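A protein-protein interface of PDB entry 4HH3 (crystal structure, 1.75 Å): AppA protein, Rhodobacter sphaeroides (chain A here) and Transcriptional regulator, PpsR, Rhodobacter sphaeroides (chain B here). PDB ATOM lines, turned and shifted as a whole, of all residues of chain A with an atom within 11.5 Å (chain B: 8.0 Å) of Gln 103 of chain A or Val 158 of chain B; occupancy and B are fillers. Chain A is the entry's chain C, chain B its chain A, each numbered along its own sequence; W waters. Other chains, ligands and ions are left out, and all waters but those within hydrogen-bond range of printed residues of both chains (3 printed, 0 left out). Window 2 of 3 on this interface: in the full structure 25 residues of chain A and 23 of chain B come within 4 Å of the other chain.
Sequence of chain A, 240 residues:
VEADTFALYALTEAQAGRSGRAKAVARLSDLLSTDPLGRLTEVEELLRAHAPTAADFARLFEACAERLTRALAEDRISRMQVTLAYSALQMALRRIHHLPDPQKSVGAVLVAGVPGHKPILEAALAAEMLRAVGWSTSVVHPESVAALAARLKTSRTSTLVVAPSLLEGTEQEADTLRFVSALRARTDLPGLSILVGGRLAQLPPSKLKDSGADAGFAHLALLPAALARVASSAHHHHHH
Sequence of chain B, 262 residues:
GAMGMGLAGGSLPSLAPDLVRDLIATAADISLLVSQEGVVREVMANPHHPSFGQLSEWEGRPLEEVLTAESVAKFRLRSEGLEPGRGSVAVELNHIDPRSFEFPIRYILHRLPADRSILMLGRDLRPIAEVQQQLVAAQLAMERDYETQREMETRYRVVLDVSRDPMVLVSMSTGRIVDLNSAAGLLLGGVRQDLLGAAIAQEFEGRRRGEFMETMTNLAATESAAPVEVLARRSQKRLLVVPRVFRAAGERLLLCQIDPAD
The guanidinium group (NE) of Arg 157 of chain B lies within salt-bridge range of the side-chain carboxylate (OD2) of Asp 161 of chain B (2.8 Å).
The side-chain carboxylate (OD1) of Asp 101 of chain A is in salt-bridge range of the guanidinium group (NE) of Arg 131 of chain A (2.9 Å).
OD2 of Asp 101 of chain A sits at hydrogen-bond distance from OG of Ser 136 of chain A (2.8 Å).
N of Thr 137 of chain A sits at hydrogen-bond distance from OD1 of Asp 101 of chain A (2.8 Å).
Of the 14 printed residues of chain B, 4 touch a printed residue of chain A.
Along chain A the printed residues that touch a printed residue of chain B span positions 100 to 103.
Water W2 lies within hydrogen-bond range of O of Asp 101 of chain A (2.6 Å) and OG1 of Thr 154 of chain B (2.9 Å).
Water W1 bridges OG1 of Thr 154 of chain B and OD2 of Asp 101 of chain A.
Water W3 bridges OD2 of Asp 161 of chain B (2.8 Å) and NE2 of Gln 103 of chain A (3.2 Å).
Gln 103 of chain A touches just these residues of chain B: Arg 157 (2.9 Å) and Val 158 (3.5 Å).
Val 158 of chain B touches one residue of chain A.
No residue of chain A comes within 4 Å of Asp 161 of chain B.
No residue of chain A comes within 4 Å of Val 162 of chain B.
No residue of chain A comes within 4 Å of Ser 163 of chain B.
Of the printed residues of chain B, Pro 100 of chain A touches Glu 153 (3.4 Å).
Of the printed residues of chain A, Glu 153 of chain B touches Pro 100 (3.4 Å).
Printed residues of chain B within 4 Å of Asp 101 of chain A: Thr 154 (3.98 Å).
Ala 108 of chain A touches none of the printed residues of chain B.
The nearest residue of chain A that does not touch Val 158 of chain B is Asp 101 of chain A (8.8 Å).
Among the printed residues, merely in contact across the chains: Pro 100 of chain A with Glu 153 of chain B (3.4 Å), Asp 101 of chain A with Thr 154 of chain B (3.98 Å), Gln 103 of chain A with Arg 157 of chain B (2.9 Å) and Gln 103 of chain A with Val 158 of chain B (3.5 Å).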
ATOM      1  N   LEU A  99      37.489   4.480   6.148  1.00  0.00           N
ATOM      2  CA  LEU A  99      36.255   4.384   6.928  1.00  0.00           C
ATOM      3  C   LEU A  99      35.324   5.564   6.755  1.00  0.00           C
ATOM      4  O   LEU A  99      35.769   6.709   6.661  1.00  0.00           O
ATOM      5  CB  LEU A  99      36.557   4.280   8.416  1.00  0.00           C
ATOM      6  CG  LEU A  99      37.179   3.001   8.951  1.00  0.00           C
ATOM      7  CD1 LEU A  99      37.590   3.244  10.398  1.00  0.00           C
ATOM      8  CD2 LEU A  99      36.195   1.856   8.871  1.00  0.00           C
ATOM      9  N   PRO A 100      34.017   5.293   6.755  1.00  0.00           N
ATOM     10  CA  PRO A 100      33.086   6.413   6.815  1.00  0.00           C
ATOM     11  C   PRO A 100      33.262   7.175   8.111  1.00  0.00           C
ATOM     12  O   PRO A 100      33.634   6.600   9.150  1.00  0.00           O
ATOM     13  CB  PRO A 100      31.712   5.728   6.804  1.00  0.00           C
ATOM     14  CG  PRO A 100      31.952   4.440   6.110  1.00  0.00           C
ATOM     15  CD  PRO A 100      33.321   4.009   6.535  1.00  0.00           C
ATOM     16  N   ASP A 101      33.013   8.476   8.051  1.00  0.00           N
ATOM     17  CA  ASP A 101      32.946   9.278   9.259  1.00  0.00           C
ATOM     18  C   ASP A 101      31.734   8.791  10.051  1.00  0.00           C
ATOM     19  O   ASP A 101      30.639   8.698   9.512  1.00  0.00           O
ATOM     20  CB  ASP A 101      32.777  10.747   8.900  1.00  0.00           C
ATOM     21  CG  ASP A 101      33.088  11.659  10.061  1.00  0.00           C
ATOM     22  OD1 ASP A 101      34.170  11.505  10.652  1.00  0.00           O
ATOM     23  OD2 ASP A 101      32.239  12.505  10.389  1.00  0.00           O
ATOM     24  N   PRO A 102      31.927   8.489  11.345  1.00  0.00           N
ATOM     25  CA  PRO A 102      30.829   7.877  12.105  1.00  0.00           C
ATOM     26  C   PRO A 102      29.700   8.859  12.443  1.00  0.00           C
ATOM     27  O   PRO A 102      29.952   9.987  12.853  1.00  0.00           O
ATOM     28  CB  PRO A 102      31.521   7.381  13.382  1.00  0.00           C
ATOM     29  CG  PRO A 102      32.705   8.264  13.544  1.00  0.00           C
ATOM     30  CD  PRO A 102      33.164   8.618  12.139  1.00  0.00           C
ATOM     31  N   GLN A 103      28.461   8.430  12.258  1.00  0.00           N
ATOM     32  CA  GLN A 103      27.316   9.288  12.563  1.00  0.00           C
ATOM     33  C   GLN A 103      26.912   9.168  14.025  1.00  0.00           C
ATOM     34  O   GLN A 103      26.441  10.132  14.628  1.00  0.00           O
ATOM     35  CB  GLN A 103      26.139   8.971  11.652  1.00  0.00           C
ATOM     36  CG  GLN A 103      26.402   9.265  10.192  1.00  0.00           C
ATOM     37  CD  GLN A 103      25.452   8.499   9.299  1.00  0.00           C
ATOM     38  OE1 GLN A 103      25.797   7.430   8.795  1.00  0.00           O
ATOM     39  NE2 GLN A 103      24.242   9.021   9.123  1.00  0.00           N
ATOM     40  N   LYS A 104      27.101   7.982  14.594  1.00  0.00           N
ATOM     41  CA  LYS A 104      26.961   7.812  16.035  1.00  0.00           C
ATOM     42  C   LYS A 104      28.329   8.069  16.648  1.00  0.00           C
ATOM     43  O   LYS A 104      29.179   7.175  16.695  1.00  0.00           O
ATOM     44  CB  LYS A 104      26.465   6.405  16.378  1.00  0.00           C
ATOM     45  CG  LYS A 104      25.092   6.087  15.817  1.00  0.00           C
ATOM     46  CD  LYS A 104      24.598   4.727  16.280  1.00  0.00           C
ATOM     47  CE  LYS A 104      23.155   4.501  15.860  1.00  0.00           C
ATOM     48  NZ  LYS A 104      22.625   3.202  16.356  1.00  0.00           N
ATOM     49  N   SER A 105      28.552   9.303  17.091  1.00  0.00           N
ATOM     50  CA  SER A 105      29.891   9.711  17.501  1.00  0.00           C
ATOM     51  C   SER A 105      30.031   9.944  19.000  1.00  0.00           C
ATOM     52  O   SER A 105      29.057  10.261  19.684  1.00  0.00           O
ATOM     53  CB  SER A 105      30.336  10.963  16.737  1.00  0.00           C
ATOM     54  OG  SER A 105      29.510  12.066  17.048  1.00  0.00           O
ATOM     55  N   VAL A 106      31.252   9.777  19.501  1.00  0.00           N
ATOM     56  CA  VAL A 106      31.547  10.041  20.901  1.00  0.00           C
ATOM     57  C   VAL A 106      32.007  11.481  21.097  1.00  0.00           C
ATOM     58  O   VAL A 106      32.141  11.944  22.227  1.00  0.00           O
ATOM     59  CB  VAL A 106      32.628   9.088  21.451  1.00  0.00           C
ATOM     60  CG1 VAL A 106      32.131   7.657  21.441  1.00  0.00           C
ATOM     61  CG2 VAL A 106      33.911   9.217  20.648  1.00  0.00           C
ATOM     62  N   GLY A 107      32.256  12.185  19.995  1.00  0.00           N
ATOM     63  CA  GLY A 107      32.710  13.567  20.051  1.00  0.00           C
ATOM     64  C   GLY A 107      33.261  13.991  18.702  1.00  0.00           C
ATOM     65  O   GLY A 107      33.290  13.179  17.781  1.00  0.00           O
ATOM     66  N   ALA A 108      33.690  15.248  18.583  1.00  0.00           N
ATOM     67  CA  ALA A 108      34.239  15.762  17.328  1.00  0.00           C
ATOM     68  C   ALA A 108      35.686  16.172  17.504  1.00  0.00           C
ATOM     69  O   ALA A 108      36.058  16.736  18.535  1.00  0.00           O
ATOM     70  CB  ALA A 108      33.432  16.952  16.830  1.00  0.00           C
ATOM     71  N   LEU A 130      40.878   7.579  14.569  1.00  0.00           N
ATOM     72  CA  LEU A 130      39.852   8.235  15.376  1.00  0.00           C
ATOM     73  C   LEU A 130      38.437   7.880  14.920  1.00  0.00           C
ATOM     74  O   LEU A 130      37.562   7.654  15.748  1.00  0.00           O
ATOM     75  CB  LEU A 130      40.043   9.753  15.372  1.00  0.00           C
ATOM     76  CG  LEU A 130      41.361  10.169  16.025  1.00  0.00           C
ATOM     77  CD1 LEU A 130      41.472  11.691  16.062  1.00  0.00           C
ATOM     78  CD2 LEU A 130      41.495   9.545  17.395  1.00  0.00           C
ATOM     79  N   ARG A 131      38.220   7.829  13.604  1.00  0.00           N
ATOM     80  CA  ARG A 131      36.950   7.369  13.057  1.00  0.00           C
ATOM     81  C   ARG A 131      36.661   5.934  13.488  1.00  0.00           C
ATOM     82  O   ARG A 131      35.501   5.581  13.765  1.00  0.00           O
ATOM     83  CB  ARG A 131      36.962   7.477  11.529  1.00  0.00           C
ATOM     84  CG  ARG A 131      36.780   8.915  11.063  1.00  0.00           C
ATOM     85  CD  ARG A 131      36.760   9.069   9.529  1.00  0.00           C
ATOM     86  NE  ARG A 131      36.401  10.453   9.223  1.00  0.00           N
ATOM     87  CZ  ARG A 131      36.913  11.174   8.226  1.00  0.00           C
ATOM     88  NH1 ARG A 131      37.789  10.644   7.382  1.00  0.00           N
ATOM     89  NH2 ARG A 131      36.517  12.434   8.068  1.00  0.00           N
ATOM     90  N   ALA A 132      37.704   5.111  13.542  1.00  0.00           N
ATOM     91  CA  ALA A 132      37.518   3.697  13.882  1.00  0.00           C
ATOM     92  C   ALA A 132      36.928   3.512  15.274  1.00  0.00           C
ATOM     93  O   ALA A 132      36.188   2.546  15.526  1.00  0.00           O
ATOM     94  CB  ALA A 132      38.828   2.911  13.729  1.00  0.00           C
ATOM     95  N   VAL A 133      37.213   4.452  16.169  1.00  0.00           N
ATOM     96  CA  VAL A 133      36.731   4.332  17.550  1.00  0.00           C
ATOM     97  C   VAL A 133      35.609   5.319  17.886  1.00  0.00           C
ATOM     98  O   VAL A 133      35.283   5.541  19.053  1.00  0.00           O
ATOM     99  CB  VAL A 133      37.888   4.410  18.568  1.00  0.00           C
ATOM    100  CG1 VAL A 133      38.918   3.329  18.266  1.00  0.00           C
ATOM    101  CG2 VAL A 133      38.541   5.789  18.555  1.00  0.00           C
ATOM    102  N   GLY A 134      34.990   5.886  16.849  1.00  0.00           N
ATOM    103  CA  GLY A 134      33.753   6.620  17.028  1.00  0.00           C
ATOM    104  C   GLY A 134      33.792   8.141  17.011  1.00  0.00           C
ATOM    105  O   GLY A 134      32.782   8.773  17.301  1.00  0.00           O
ATOM    106  N   TRP A 135      34.926   8.739  16.658  1.00  0.00           N
ATOM    107  CA  TRP A 135      35.005  10.200  16.613  1.00  0.00           C
ATOM    108  C   TRP A 135      34.641  10.752  15.242  1.00  0.00           C
ATOM    109  O   TRP A 135      35.190  10.309  14.248  1.00  0.00           O
ATOM    110  CB  TRP A 135      36.416  10.669  16.947  1.00  0.00           C
ATOM    111  CG  TRP A 135      36.752  10.500  18.391  1.00  0.00           C
ATOM    112  CD1 TRP A 135      37.192   9.365  19.004  1.00  0.00           C
ATOM    113  CD2 TRP A 135      36.681  11.505  19.406  1.00  0.00           C
ATOM    114  NE1 TRP A 135      37.392   9.598  20.346  1.00  0.00           N
ATOM    115  CE2 TRP A 135      37.085  10.905  20.618  1.00  0.00           C
ATOM    116  CE3 TRP A 135      36.323  12.858  19.407  1.00  0.00           C
ATOM    117  CZ2 TRP A 135      37.142  11.614  21.818  1.00  0.00           C
ATOM    118  CZ3 TRP A 135      36.377  13.559  20.604  1.00  0.00           C
ATOM    119  CH2 TRP A 135      36.780  12.934  21.791  1.00  0.00           C
ATOM    120  N   SER A 136      33.730  11.722  15.202  1.00  0.00           N
ATOM    121  CA  SER A 136      33.496  12.460  13.969  1.00  0.00           C
ATOM    122  C   SER A 136      34.704  13.348  13.753  1.00  0.00           C
ATOM    123  O   SER A 136      35.074  14.134  14.624  1.00  0.00           O
ATOM    124  CB  SER A 136      32.230  13.307  14.044  1.00  0.00           C
ATOM    125  OG  SER A 136      31.997  13.932  12.788  1.00  0.00           O
ATOM    126  N   THR A 137      35.312  13.230  12.584  1.00  0.00           N
ATOM    127  CA  THR A 137      36.649  13.777  12.391  1.00  0.00           C
ATOM    128  C   THR A 137      36.695  14.631  11.132  1.00  0.00           C
ATOM    129  O   THR A 137      36.004  14.361  10.149  1.00  0.00           O
ATOM    130  CB  THR A 137      37.689  12.628  12.278  1.00  0.00           C
ATOM    131  OG1 THR A 137      37.604  11.783  13.436  1.00  0.00           O
ATOM    132  CG2 THR A 137      39.134  13.169  12.146  1.00  0.00           C
ATOM    133  N   GLU B 151      32.309  13.749   3.433  1.00  0.00           N
ATOM    134  CA  GLU B 151      31.120  14.577   3.670  1.00  0.00           C
ATOM    135  C   GLU B 151      29.954  14.046   2.853  1.00  0.00           C
ATOM    136  O   GLU B 151      28.847  13.850   3.373  1.00  0.00           O
ATOM    137  CB  GLU B 151      31.318  16.044   3.292  1.00  0.00           C
ATOM    138  CG  GLU B 151      30.087  16.873   3.682  1.00  0.00           C
ATOM    139  CD  GLU B 151      30.019  18.266   3.095  1.00  0.00           C
ATOM    140  OE1 GLU B 151      31.045  18.784   2.594  1.00  0.00           O
ATOM    141  OE2 GLU B 151      28.914  18.846   3.157  1.00  0.00           O
ATOM    142  N   MET B 152      30.211  13.808   1.573  1.00  0.00           N
ATOM    143  CA  MET B 152      29.149  13.328   0.688  1.00  0.00           C
ATOM    144  C   MET B 152      28.614  11.962   1.105  1.00  0.00           C
ATOM    145  O   MET B 152      27.413  11.706   0.960  1.00  0.00           O
ATOM    146  CB  MET B 152      29.630  13.290  -0.756  1.00  0.00           C
ATOM    147  CG  MET B 152      30.021  14.656  -1.249  1.00  0.00           C
ATOM    148  SD  MET B 152      28.634  15.818  -1.184  1.00  0.00           S
ATOM    149  CE  MET B 152      29.521  17.364  -0.962  1.00  0.00           C
ATOM    150  N   GLU B 153      29.485  11.078   1.595  1.00  0.00           N
ATOM    151  CA  GLU B 153      29.029   9.768   2.070  1.00  0.00           C
ATOM    152  C   GLU B 153      28.043   9.890   3.231  1.00  0.00           C
ATOM    153  O   GLU B 153      27.047   9.168   3.284  1.00  0.00           O
ATOM    154  CB  GLU B 153      30.208   8.868   2.460  1.00  0.00           C
ATOM    155  CG  GLU B 153      29.761   7.564   3.124  1.00  0.00           C
ATOM    156  CD  GLU B 153      30.792   6.450   3.096  1.00  0.00           C
ATOM    157  OE1 GLU B 153      30.382   5.269   3.228  1.00  0.00           O
ATOM    158  OE2 GLU B 153      31.998   6.733   2.968  1.00  0.00           O
ATOM    159  N   THR B 154      28.311  10.793   4.175  1.00  0.00           N
ATOM    160  CA  THR B 154      27.355  11.006   5.262  1.00  0.00           C
ATOM    161  C   THR B 154      26.047  11.581   4.725  1.00  0.00           C
ATOM    162  O   THR B 154      24.967  11.169   5.147  1.00  0.00           O
ATOM    163  CB  THR B 154      27.911  11.929   6.356  1.00  0.00           C
ATOM    164  OG1 THR B 154      29.048  11.295   6.954  1.00  0.00           O
ATOM    165  CG2 THR B 154      26.859  12.173   7.433  1.00  0.00           C
ATOM    166  N   ARG B 155      26.144  12.523   3.788  1.00  0.00           N
ATOM    167  CA  ARG B 155      24.921  13.085   3.190  1.00  0.00           C
ATOM    168  C   ARG B 155      24.102  11.988   2.524  1.00  0.00           C
ATOM    169  O   ARG B 155      22.876  11.924   2.685  1.00  0.00           O
ATOM    170  CB  ARG B 155      25.254  14.148   2.140  1.00  0.00           C
ATOM    171  CG  ARG B 155      25.842  15.456   2.666  1.00  0.00           C
ATOM    172  CD  ARG B 155      25.679  16.467   1.535  1.00  0.00           C
ATOM    173  NE  ARG B 155      26.510  17.643   1.667  1.00  0.00           N
ATOM    174  CZ  ARG B 155      26.478  18.648   0.805  1.00  0.00           C
ATOM    175  NH1 ARG B 155      25.629  18.615  -0.222  1.00  0.00           N
ATOM    176  NH2 ARG B 155      27.278  19.686   0.972  1.00  0.00           N
ATOM    177  N   TYR B 156      24.778  11.144   1.751  1.00  0.00           N
ATOM    178  CA  TYR B 156      24.141   9.975   1.116  1.00  0.00           C
ATOM    179  C   TYR B 156      23.428   9.075   2.129  1.00  0.00           C
ATOM    180  O   TYR B 156      22.244   8.730   1.962  1.00  0.00           O
ATOM    181  CB  TYR B 156      25.210   9.183   0.356  1.00  0.00           C
ATOM    182  CG  TYR B 156      24.876   7.737   0.048  1.00  0.00           C
ATOM    183  CD1 TYR B 156      24.057   7.412  -1.027  1.00  0.00           C
ATOM    184  CD2 TYR B 156      25.427   6.703   0.792  1.00  0.00           C
ATOM    185  CE1 TYR B 156      23.770   6.077  -1.331  1.00  0.00           C
ATOM    186  CE2 TYR B 156      25.147   5.371   0.503  1.00  0.00           C
ATOM    187  CZ  TYR B 156      24.316   5.071  -0.564  1.00  0.00           C
ATOM    188  OH  TYR B 156      24.051   3.760  -0.861  1.00  0.00           O
ATOM    189  N   ARG B 157      24.149   8.713   3.180  1.00  0.00           N
ATOM    190  CA  ARG B 157      23.616   7.845   4.230  1.00  0.00           C
ATOM    191  C   ARG B 157      22.333   8.427   4.832  1.00  0.00           C
ATOM    192  O   ARG B 157      21.310   7.726   4.936  1.00  0.00           O
ATOM    193  CB  ARG B 157      24.698   7.639   5.299  1.00  0.00           C
ATOM    194  CG  ARG B 157      24.347   6.697   6.410  1.00  0.00           C
ATOM    195  CD  ARG B 157      24.565   5.255   6.013  1.00  0.00           C
ATOM    196  NE  ARG B 157      23.333   4.697   5.478  1.00  0.00           N
ATOM    197  CZ  ARG B 157      23.262   3.922   4.407  1.00  0.00           C
ATOM    198  NH1 ARG B 157      24.361   3.606   3.739  1.00  0.00           N
ATOM    199  NH2 ARG B 157      22.080   3.468   4.013  1.00  0.00           N
ATOM    200  N   VAL B 158      22.375   9.709   5.194  1.00  0.00           N
ATOM    201  CA  VAL B 158      21.217  10.366   5.800  1.00  0.00           C
ATOM    202  C   VAL B 158      20.041  10.499   4.834  1.00  0.00           C
ATOM    203  O   VAL B 158      18.909  10.163   5.178  1.00  0.00           O
ATOM    204  CB  VAL B 158      21.569  11.741   6.382  1.00  0.00           C
ATOM    205  CG1 VAL B 158      20.304  12.475   6.830  1.00  0.00           C
ATOM    206  CG2 VAL B 158      22.534  11.575   7.543  1.00  0.00           C
ATOM    207  N   VAL B 159      20.307  10.985   3.628  1.00  0.00           N
ATOM    208  CA  VAL B 159      19.248  11.086   2.622  1.00  0.00           C
ATOM    209  C   VAL B 159      18.600   9.735   2.345  1.00  0.00           C
ATOM    210  O   VAL B 159      17.371   9.621   2.357  1.00  0.00           O
ATOM    211  CB  VAL B 159      19.774  11.734   1.308  1.00  0.00           C
ATOM    212  CG1 VAL B 159      18.738  11.601   0.174  1.00  0.00           C
ATOM    213  CG2 VAL B 159      20.092  13.209   1.541  1.00  0.00           C
ATOM    214  N   LEU B 160      19.407   8.712   2.097  1.00  0.00           N
ATOM    215  CA  LEU B 160      18.861   7.383   1.807  1.00  0.00           C
ATOM    216  C   LEU B 160      18.027   6.854   2.976  1.00  0.00           C
ATOM    217  O   LEU B 160      16.885   6.412   2.796  1.00  0.00           O
ATOM    218  CB  LEU B 160      19.987   6.405   1.465  1.00  0.00           C
ATOM    219  CG  LEU B 160      19.596   4.941   1.218  1.00  0.00           C
ATOM    220  CD1 LEU B 160      18.549   4.857   0.107  1.00  0.00           C
ATOM    221  CD2 LEU B 160      20.824   4.107   0.855  1.00  0.00           C
ATOM    222  N   ASP B 161      18.591   6.917   4.179  1.00  0.00           N
ATOM    223  CA  ASP B 161      17.933   6.332   5.353  1.00  0.00           C
ATOM    224  C   ASP B 161      16.649   7.061   5.746  1.00  0.00           C
ATOM    225  O   ASP B 161      15.654   6.422   6.109  1.00  0.00           O
ATOM    226  CB  ASP B 161      18.890   6.289   6.549  1.00  0.00           C
ATOM    227  CG  ASP B 161      20.023   5.283   6.369  1.00  0.00           C
ATOM    228  OD1 ASP B 161      19.843   4.282   5.643  1.00  0.00           O
ATOM    229  OD2 ASP B 161      21.101   5.489   6.974  1.00  0.00           O
ATOM    230  N   VAL B 162      16.664   8.387   5.671  1.00  0.00           N
ATOM    231  CA  VAL B 162      15.504   9.186   6.057  1.00  0.00           C
ATOM    232  C   VAL B 162      14.410   9.188   4.976  1.00  0.00           C
ATOM    233  O   VAL B 162      13.228   9.304   5.293  1.00  0.00           O
ATOM    234  CB  VAL B 162      15.920  10.630   6.426  1.00  0.00           C
ATOM    235  CG1 VAL B 162      14.720  11.524   6.698  1.00  0.00           C
ATOM    236  CG2 VAL B 162      16.850  10.621   7.658  1.00  0.00           C
ATOM    237  N   SER B 163      14.799   9.049   3.710  1.00  0.00           N
ATOM    238  CA  SER B 163      13.831   9.111   2.608  1.00  0.00           C
ATOM    239  C   SER B 163      12.700   8.105   2.745  1.00  0.00           C
ATOM    240  O   SER B 163      12.936   6.915   2.955  1.00  0.00           O
ATOM    241  CB  SER B 163      14.501   8.877   1.256  1.00  0.00           C
ATOM    242  OG  SER B 163      13.534   8.987   0.209  1.00  0.00           O
ATOM    243  N   ASN B 181      17.166   1.272   1.982  1.00  0.00           N
ATOM    244  CA  ASN B 181      16.664   1.959   3.170  1.00  0.00           C
ATOM    245  C   ASN B 181      15.578   1.150   3.887  1.00  0.00           C
ATOM    246  O   ASN B 181      15.120   0.116   3.367  1.00  0.00           O
ATOM    247  CB  ASN B 181      16.221   3.405   2.877  1.00  0.00           C
ATOM    248  CG  ASN B 181      15.117   3.508   1.825  1.00  0.00           C
ATOM    249  OD1 ASN B 181      14.495   2.507   1.426  1.00  0.00           O
ATOM    250  ND2 ASN B 181      14.855   4.747   1.377  1.00  0.00           N
HETATM  251  O   HOH W   1      29.597  12.025   9.536  1.00  0.00           O
HETATM  252  O   HOH W   2      29.619   8.498   7.101  1.00  0.00           O
HETATM  253  O   HOH W   3      21.384   7.765   8.628  1.00  0.00           O
